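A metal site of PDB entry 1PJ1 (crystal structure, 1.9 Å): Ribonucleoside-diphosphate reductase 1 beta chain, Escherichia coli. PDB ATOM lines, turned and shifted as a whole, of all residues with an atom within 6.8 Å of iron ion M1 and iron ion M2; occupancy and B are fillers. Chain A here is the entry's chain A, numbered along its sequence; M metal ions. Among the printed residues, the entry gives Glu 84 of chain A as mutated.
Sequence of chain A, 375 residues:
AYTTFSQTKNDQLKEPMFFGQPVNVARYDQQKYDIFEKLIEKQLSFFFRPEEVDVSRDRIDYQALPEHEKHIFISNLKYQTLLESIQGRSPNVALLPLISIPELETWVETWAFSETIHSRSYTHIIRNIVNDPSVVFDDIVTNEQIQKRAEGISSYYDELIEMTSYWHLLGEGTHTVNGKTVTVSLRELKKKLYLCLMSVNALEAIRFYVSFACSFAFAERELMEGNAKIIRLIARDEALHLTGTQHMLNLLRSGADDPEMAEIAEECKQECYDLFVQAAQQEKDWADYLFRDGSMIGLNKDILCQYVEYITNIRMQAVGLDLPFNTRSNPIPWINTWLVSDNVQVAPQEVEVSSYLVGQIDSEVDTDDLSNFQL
The backbone carbonyl oxygen of Glu 115 lies within hydrogen-bond range of the side-chain hydroxyl of Ser 119 (3.4 Å). O of Glu 84 sits close to OG of Ser 119, at 3.5 Å. NE2 of His 118 sits close to O of Ser 114. NE2 of His 118 lies within hydrogen-bond range of OD2 of Asp 237, 2.6 Å away. The indole nitrogen (NE1) of Trp 111 sits close to the side-chain carboxylate (OE2) of Glu 115 (3.3 Å). A ring nitrogen (NE2) of His 241 is in hydrogen-bond range of the side-chain hydroxyl of Ser 114 (2.8 Å). O of Trp 111 sits at hydrogen-bond distance from OG of Ser 114, 2.6 Å away. OE2 of Glu 204 sits at hydrogen-bond distance from NE2 of Gln 87 (2.8 Å).
Trp 111 touches iron ion M1 (NE1 to FE, 3.7 Å). Phe 208 touches iron ion M1 (CE2 to FE, 3.8 Å). Of the 20 residues printed, 6 come within 4 Å of iron ion M1.
Phe 208 touches iron ion M2. Five residues have an atom within 4 Å of iron ion M2: Glu 84, Glu 115, His 118, Phe 208 and Glu 238. Along chain A the residues within 4 Å of iron ion M2 span positions 84 to 238. The nearest printed residue that does not touch iron ion M2 is Ile 234 (4.2 Å).
Iron ion M1 is bound by OE2 of Glu 115 (2.0 Å), OE1 of Glu 238 (2.0 Å), OE1 of Glu 204 (2.0 Å) and ND1 of His 241 (2.0 Å).
Iron ion M2 is bound by OE2 of Glu 238 (2.0 Å), ND1 of His 118 (2.1 Å), OE1 of Glu 115 (2.1 Å), OE2 of Glu 84 (2.2 Å) and OE1 of Glu 84 (2.2 Å). Iron ion M2 has five donor atoms within binding distance.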
ATOM      1  N   GLN A  80     -18.935  15.722  11.040  1.00  0.00           N
ATOM      2  CA  GLN A  80     -19.100  16.089  12.446  1.00  0.00           C
ATOM      3  C   GLN A  80     -19.542  17.549  12.527  1.00  0.00           C
ATOM      4  O   GLN A  80     -20.439  17.900  13.297  1.00  0.00           O
ATOM      5  CB  GLN A  80     -17.786  15.896  13.220  1.00  0.00           C
ATOM      6  CG  GLN A  80     -17.243  14.456  13.216  1.00  0.00           C
ATOM      7  CD  GLN A  80     -15.889  14.308  13.911  1.00  0.00           C
ATOM      8  OE1 GLN A  80     -14.967  15.096  13.685  1.00  0.00           O
ATOM      9  NE2 GLN A  80     -15.757  13.294  14.759  1.00  0.00           N
ATOM     10  N   LEU A  83     -23.225  17.873  11.624  1.00  0.00           N
ATOM     11  CA  LEU A  83     -24.100  17.471  12.726  1.00  0.00           C
ATOM     12  C   LEU A  83     -24.142  18.488  13.867  1.00  0.00           C
ATOM     13  O   LEU A  83     -25.209  18.710  14.459  1.00  0.00           O
ATOM     14  CB  LEU A  83     -23.695  16.103  13.275  1.00  0.00           C
ATOM     15  CG  LEU A  83     -23.815  14.896  12.334  1.00  0.00           C
ATOM     16  CD1 LEU A  83     -23.432  13.638  13.099  1.00  0.00           C
ATOM     17  CD2 LEU A  83     -25.245  14.779  11.814  1.00  0.00           C
ATOM     18  N   GLU A  84     -23.007  19.105  14.181  1.00  0.00           N
ATOM     19  CA  GLU A  84     -22.981  20.096  15.266  1.00  0.00           C
ATOM     20  C   GLU A  84     -23.738  21.359  14.854  1.00  0.00           C
ATOM     21  O   GLU A  84     -24.406  21.979  15.685  1.00  0.00           O
ATOM     22  CB  GLU A  84     -21.526  20.445  15.646  1.00  0.00           C
ATOM     23  CG  GLU A  84     -20.717  19.262  16.160  1.00  0.00           C
ATOM     24  CD  GLU A  84     -21.216  18.703  17.479  1.00  0.00           C
ATOM     25  OE1 GLU A  84     -22.292  19.124  17.961  1.00  0.00           O
ATOM     26  OE2 GLU A  84     -20.516  17.831  18.043  1.00  0.00           O
ATOM     27  N   GLN A  87     -27.280  20.386  15.362  1.00  0.00           N
ATOM     28  CA  GLN A  87     -27.619  20.189  16.774  1.00  0.00           C
ATOM     29  C   GLN A  87     -27.502  21.445  17.636  1.00  0.00           C
ATOM     30  O   GLN A  87     -28.065  21.504  18.729  1.00  0.00           O
ATOM     31  CB  GLN A  87     -26.761  19.063  17.365  1.00  0.00           C
ATOM     32  CG  GLN A  87     -27.197  17.669  16.885  1.00  0.00           C
ATOM     33  CD  GLN A  87     -28.692  17.436  17.060  1.00  0.00           C
ATOM     34  OE1 GLN A  87     -29.493  17.842  16.214  1.00  0.00           O
ATOM     35  NE2 GLN A  87     -29.072  16.812  18.164  1.00  0.00           N
ATOM     36  N   TRP A 111     -28.063  21.805  26.486  1.00  0.00           N
ATOM     37  CA  TRP A 111     -27.617  20.766  25.579  1.00  0.00           C
ATOM     38  C   TRP A 111     -27.249  21.426  24.240  1.00  0.00           C
ATOM     39  O   TRP A 111     -26.130  21.280  23.734  1.00  0.00           O
ATOM     40  CB  TRP A 111     -28.752  19.732  25.459  1.00  0.00           C
ATOM     41  CG  TRP A 111     -28.776  18.835  24.269  1.00  0.00           C
ATOM     42  CD1 TRP A 111     -27.737  18.493  23.447  1.00  0.00           C
ATOM     43  CD2 TRP A 111     -29.915  18.113  23.804  1.00  0.00           C
ATOM     44  NE1 TRP A 111     -28.166  17.592  22.497  1.00  0.00           N
ATOM     45  CE2 TRP A 111     -29.499  17.342  22.694  1.00  0.00           C
ATOM     46  CE3 TRP A 111     -31.259  18.026  24.220  1.00  0.00           C
ATOM     47  CZ2 TRP A 111     -30.375  16.505  21.990  1.00  0.00           C
ATOM     48  CZ3 TRP A 111     -32.135  17.189  23.516  1.00  0.00           C
ATOM     49  CH2 TRP A 111     -31.687  16.442  22.419  1.00  0.00           C
ATOM     50  N   SER A 114     -24.079  23.550  24.344  1.00  0.00           N
ATOM     51  CA  SER A 114     -22.840  22.767  24.323  1.00  0.00           C
ATOM     52  C   SER A 114     -22.502  22.348  22.892  1.00  0.00           C
ATOM     53  O   SER A 114     -21.327  22.250  22.529  1.00  0.00           O
ATOM     54  CB  SER A 114     -22.957  21.543  25.247  1.00  0.00           C
ATOM     55  OG  SER A 114     -23.800  20.538  24.723  1.00  0.00           O
ATOM     56  N   GLU A 115     -23.520  22.119  22.071  1.00  0.00           N
ATOM     57  CA  GLU A 115     -23.279  21.726  20.679  1.00  0.00           C
ATOM     58  C   GLU A 115     -22.640  22.897  19.909  1.00  0.00           C
ATOM     59  O   GLU A 115     -21.815  22.681  19.012  1.00  0.00           O
ATOM     60  CB  GLU A 115     -24.582  21.280  20.001  1.00  0.00           C
ATOM     61  CG  GLU A 115     -25.366  20.210  20.780  1.00  0.00           C
ATOM     62  CD  GLU A 115     -24.754  18.814  20.714  1.00  0.00           C
ATOM     63  OE1 GLU A 115     -23.515  18.694  20.775  1.00  0.00           O
ATOM     64  OE2 GLU A 115     -25.521  17.832  20.612  1.00  0.00           O
ATOM     65  N   THR A 116     -22.989  24.142  20.252  1.00  0.00           N
ATOM     66  CA  THR A 116     -22.389  25.277  19.566  1.00  0.00           C
ATOM     67  C   THR A 116     -20.918  25.376  19.953  1.00  0.00           C
ATOM     68  O   THR A 116     -20.085  25.832  19.165  1.00  0.00           O
ATOM     69  CB  THR A 116     -23.098  26.621  19.877  1.00  0.00           C
ATOM     70  OG1 THR A 116     -22.911  26.962  21.256  1.00  0.00           O
ATOM     71  CG2 THR A 116     -24.583  26.511  19.563  1.00  0.00           C
ATOM     72  N   HIS A 118     -19.154  22.808  20.485  1.00  0.00           N
ATOM     73  CA  HIS A 118     -18.552  21.766  19.662  1.00  0.00           C
ATOM     74  C   HIS A 118     -18.310  22.319  18.251  1.00  0.00           C
ATOM     75  O   HIS A 118     -17.284  22.035  17.636  1.00  0.00           O
ATOM     76  CB  HIS A 118     -19.478  20.549  19.621  1.00  0.00           C
ATOM     77  CG  HIS A 118     -19.720  19.930  20.961  1.00  0.00           C
ATOM     78  ND1 HIS A 118     -20.590  18.893  21.157  1.00  0.00           N
ATOM     79  CD2 HIS A 118     -19.211  20.235  22.180  1.00  0.00           C
ATOM     80  CE1 HIS A 118     -20.616  18.576  22.447  1.00  0.00           C
ATOM     81  NE2 HIS A 118     -19.788  19.372  23.083  1.00  0.00           N
ATOM     82  N   SER A 119     -19.245  23.119  17.752  1.00  0.00           N
ATOM     83  CA  SER A 119     -19.067  23.727  16.426  1.00  0.00           C
ATOM     84  C   SER A 119     -17.860  24.650  16.435  1.00  0.00           C
ATOM     85  O   SER A 119     -17.061  24.659  15.494  1.00  0.00           O
ATOM     86  CB  SER A 119     -20.315  24.526  16.023  1.00  0.00           C
ATOM     87  OG  SER A 119     -21.396  23.672  15.748  1.00  0.00           O
ATOM     88  N   TYR A 122     -14.651  22.743  16.170  1.00  0.00           N
ATOM     89  CA  TYR A 122     -14.298  22.329  14.820  1.00  0.00           C
ATOM     90  C   TYR A 122     -13.749  23.467  13.952  1.00  0.00           C
ATOM     91  O   TYR A 122     -12.904  23.234  13.087  1.00  0.00           O
ATOM     92  CB  TYR A 122     -15.491  21.644  14.150  1.00  0.00           C
ATOM     93  CG  TYR A 122     -15.748  20.270  14.722  1.00  0.00           C
ATOM     94  CD1 TYR A 122     -14.742  19.296  14.710  1.00  0.00           C
ATOM     95  CD2 TYR A 122     -16.982  19.928  15.296  1.00  0.00           C
ATOM     96  CE1 TYR A 122     -14.960  18.021  15.253  1.00  0.00           C
ATOM     97  CE2 TYR A 122     -17.199  18.662  15.843  1.00  0.00           C
ATOM     98  CZ  TYR A 122     -16.183  17.714  15.820  1.00  0.00           C
ATOM     99  OH  TYR A 122     -16.378  16.455  16.348  1.00  0.00           O
ATOM    100  N   GLU A 204     -27.307  11.329  18.263  1.00  0.00           N
ATOM    101  CA  GLU A 204     -26.418  11.534  19.396  1.00  0.00           C
ATOM    102  C   GLU A 204     -25.647  10.270  19.807  1.00  0.00           C
ATOM    103  O   GLU A 204     -24.445  10.322  20.074  1.00  0.00           O
ATOM    104  CB  GLU A 204     -27.221  12.009  20.629  1.00  0.00           C
ATOM    105  CG  GLU A 204     -27.985  13.325  20.478  1.00  0.00           C
ATOM    106  CD  GLU A 204     -27.099  14.555  20.618  1.00  0.00           C
ATOM    107  OE1 GLU A 204     -25.964  14.432  21.103  1.00  0.00           O
ATOM    108  OE2 GLU A 204     -27.560  15.659  20.238  1.00  0.00           O
ATOM    109  N   PHE A 208     -22.605  10.273  16.032  1.00  0.00           N
ATOM    110  CA  PHE A 208     -21.436  10.933  16.618  1.00  0.00           C
ATOM    111  C   PHE A 208     -20.340   9.920  16.991  1.00  0.00           C
ATOM    112  O   PHE A 208     -19.158  10.147  16.737  1.00  0.00           O
ATOM    113  CB  PHE A 208     -21.798  11.737  17.879  1.00  0.00           C
ATOM    114  CG  PHE A 208     -22.328  13.123  17.599  1.00  0.00           C
ATOM    115  CD1 PHE A 208     -21.675  13.966  16.697  1.00  0.00           C
ATOM    116  CD2 PHE A 208     -23.461  13.601  18.255  1.00  0.00           C
ATOM    117  CE1 PHE A 208     -22.142  15.269  16.459  1.00  0.00           C
ATOM    118  CE2 PHE A 208     -23.929  14.898  18.029  1.00  0.00           C
ATOM    119  CZ  PHE A 208     -23.270  15.728  17.129  1.00  0.00           C
ATOM    120  N   PHE A 212     -16.312   9.400  16.068  1.00  0.00           N
ATOM    121  CA  PHE A 212     -15.255   9.448  17.071  1.00  0.00           C
ATOM    122  C   PHE A 212     -14.213   8.366  16.813  1.00  0.00           C
ATOM    123  O   PHE A 212     -13.014   8.598  16.985  1.00  0.00           O
ATOM    124  CB  PHE A 212     -15.820   9.275  18.485  1.00  0.00           C
ATOM    125  CG  PHE A 212     -16.723  10.387  18.928  1.00  0.00           C
ATOM    126  CD1 PHE A 212     -16.621  11.644  18.356  1.00  0.00           C
ATOM    127  CD2 PHE A 212     -17.662  10.184  19.934  1.00  0.00           C
ATOM    128  CE1 PHE A 212     -17.453  12.692  18.779  1.00  0.00           C
ATOM    129  CE2 PHE A 212     -18.483  11.206  20.361  1.00  0.00           C
ATOM    130  CZ  PHE A 212     -18.388  12.466  19.782  1.00  0.00           C
ATOM    131  N   ILE A 234     -15.621  16.537  23.532  1.00  0.00           N
ATOM    132  CA  ILE A 234     -16.911  16.481  22.852  1.00  0.00           C
ATOM    133  C   ILE A 234     -17.642  15.198  23.227  1.00  0.00           C
ATOM    134  O   ILE A 234     -18.809  15.241  23.611  1.00  0.00           O
ATOM    135  CB  ILE A 234     -16.732  16.581  21.332  1.00  0.00           C
ATOM    136  CG1 ILE A 234     -16.175  17.961  20.980  1.00  0.00           C
ATOM    137  CG2 ILE A 234     -18.072  16.324  20.616  1.00  0.00           C
ATOM    138  CD1 ILE A 234     -15.928  18.159  19.493  1.00  0.00           C
ATOM    139  N   ASP A 237     -19.454  15.229  26.375  1.00  0.00           N
ATOM    140  CA  ASP A 237     -20.754  15.919  26.325  1.00  0.00           C
ATOM    141  C   ASP A 237     -21.818  15.042  25.656  1.00  0.00           C
ATOM    142  O   ASP A 237     -22.942  14.940  26.145  1.00  0.00           O
ATOM    143  CB  ASP A 237     -20.640  17.237  25.555  1.00  0.00           C
ATOM    144  CG  ASP A 237     -19.792  18.277  26.285  1.00  0.00           C
ATOM    145  OD1 ASP A 237     -19.606  18.146  27.509  1.00  0.00           O
ATOM    146  OD2 ASP A 237     -19.352  19.243  25.636  1.00  0.00           O
ATOM    147  N   GLU A 238     -21.466  14.405  24.537  1.00  0.00           N
ATOM    148  CA  GLU A 238     -22.427  13.569  23.829  1.00  0.00           C
ATOM    149  C   GLU A 238     -22.994  12.459  24.732  1.00  0.00           C
ATOM    150  O   GLU A 238     -24.149  12.046  24.578  1.00  0.00           O
ATOM    151  CB  GLU A 238     -21.804  12.946  22.572  1.00  0.00           C
ATOM    152  CG  GLU A 238     -21.222  13.927  21.560  1.00  0.00           C
ATOM    153  CD  GLU A 238     -22.180  15.045  21.148  1.00  0.00           C
ATOM    154  OE1 GLU A 238     -23.403  14.900  21.355  1.00  0.00           O
ATOM    155  OE2 GLU A 238     -21.690  16.069  20.624  1.00  0.00           O
ATOM    156  N   ALA A 239     -22.173  11.975  25.667  1.00  0.00           N
ATOM    157  CA  ALA A 239     -22.619  10.931  26.592  1.00  0.00           C
ATOM    158  C   ALA A 239     -23.782  11.450  27.446  1.00  0.00           C
ATOM    159  O   ALA A 239     -24.734  10.706  27.747  1.00  0.00           O
ATOM    160  CB  ALA A 239     -21.473  10.492  27.476  1.00  0.00           C
ATOM    161  N   HIS A 241     -25.787  13.982  26.534  1.00  0.00           N
ATOM    162  CA  HIS A 241     -26.898  14.221  25.618  1.00  0.00           C
ATOM    163  C   HIS A 241     -27.702  12.953  25.354  1.00  0.00           C
ATOM    164  O   HIS A 241     -28.930  12.971  25.410  1.00  0.00           O
ATOM    165  CB  HIS A 241     -26.383  14.793  24.291  1.00  0.00           C
ATOM    166  CG  HIS A 241     -25.593  16.054  24.457  1.00  0.00           C
ATOM    167  ND1 HIS A 241     -24.865  16.614  23.432  1.00  0.00           N
ATOM    168  CD2 HIS A 241     -25.408  16.865  25.534  1.00  0.00           C
ATOM    169  CE1 HIS A 241     -24.256  17.702  23.860  1.00  0.00           C
ATOM    170  NE2 HIS A 241     -24.570  17.885  25.125  1.00  0.00           N
ATOM    171  N   LEU A 242     -27.025  11.852  25.079  1.00  0.00           N
ATOM    172  CA  LEU A 242     -27.740  10.623  24.806  1.00  0.00           C
ATOM    173  C   LEU A 242     -28.381  10.073  26.091  1.00  0.00           C
ATOM    174  O   LEU A 242     -29.418   9.417  26.046  1.00  0.00           O
ATOM    175  CB  LEU A 242     -26.823   9.592  24.144  1.00  0.00           C
ATOM    176  CG  LEU A 242     -25.753   8.843  24.924  1.00  0.00           C
ATOM    177  CD1 LEU A 242     -26.390   7.690  25.702  1.00  0.00           C
ATOM    178  CD2 LEU A 242     -24.706   8.307  23.946  1.00  0.00           C
HETATM  179 FE    FE M   1     -24.971  16.128  21.455  1.00  0.00          FE
HETATM  180 FE    FE M   2     -21.836  17.894  19.786  1.00  0.00          FE
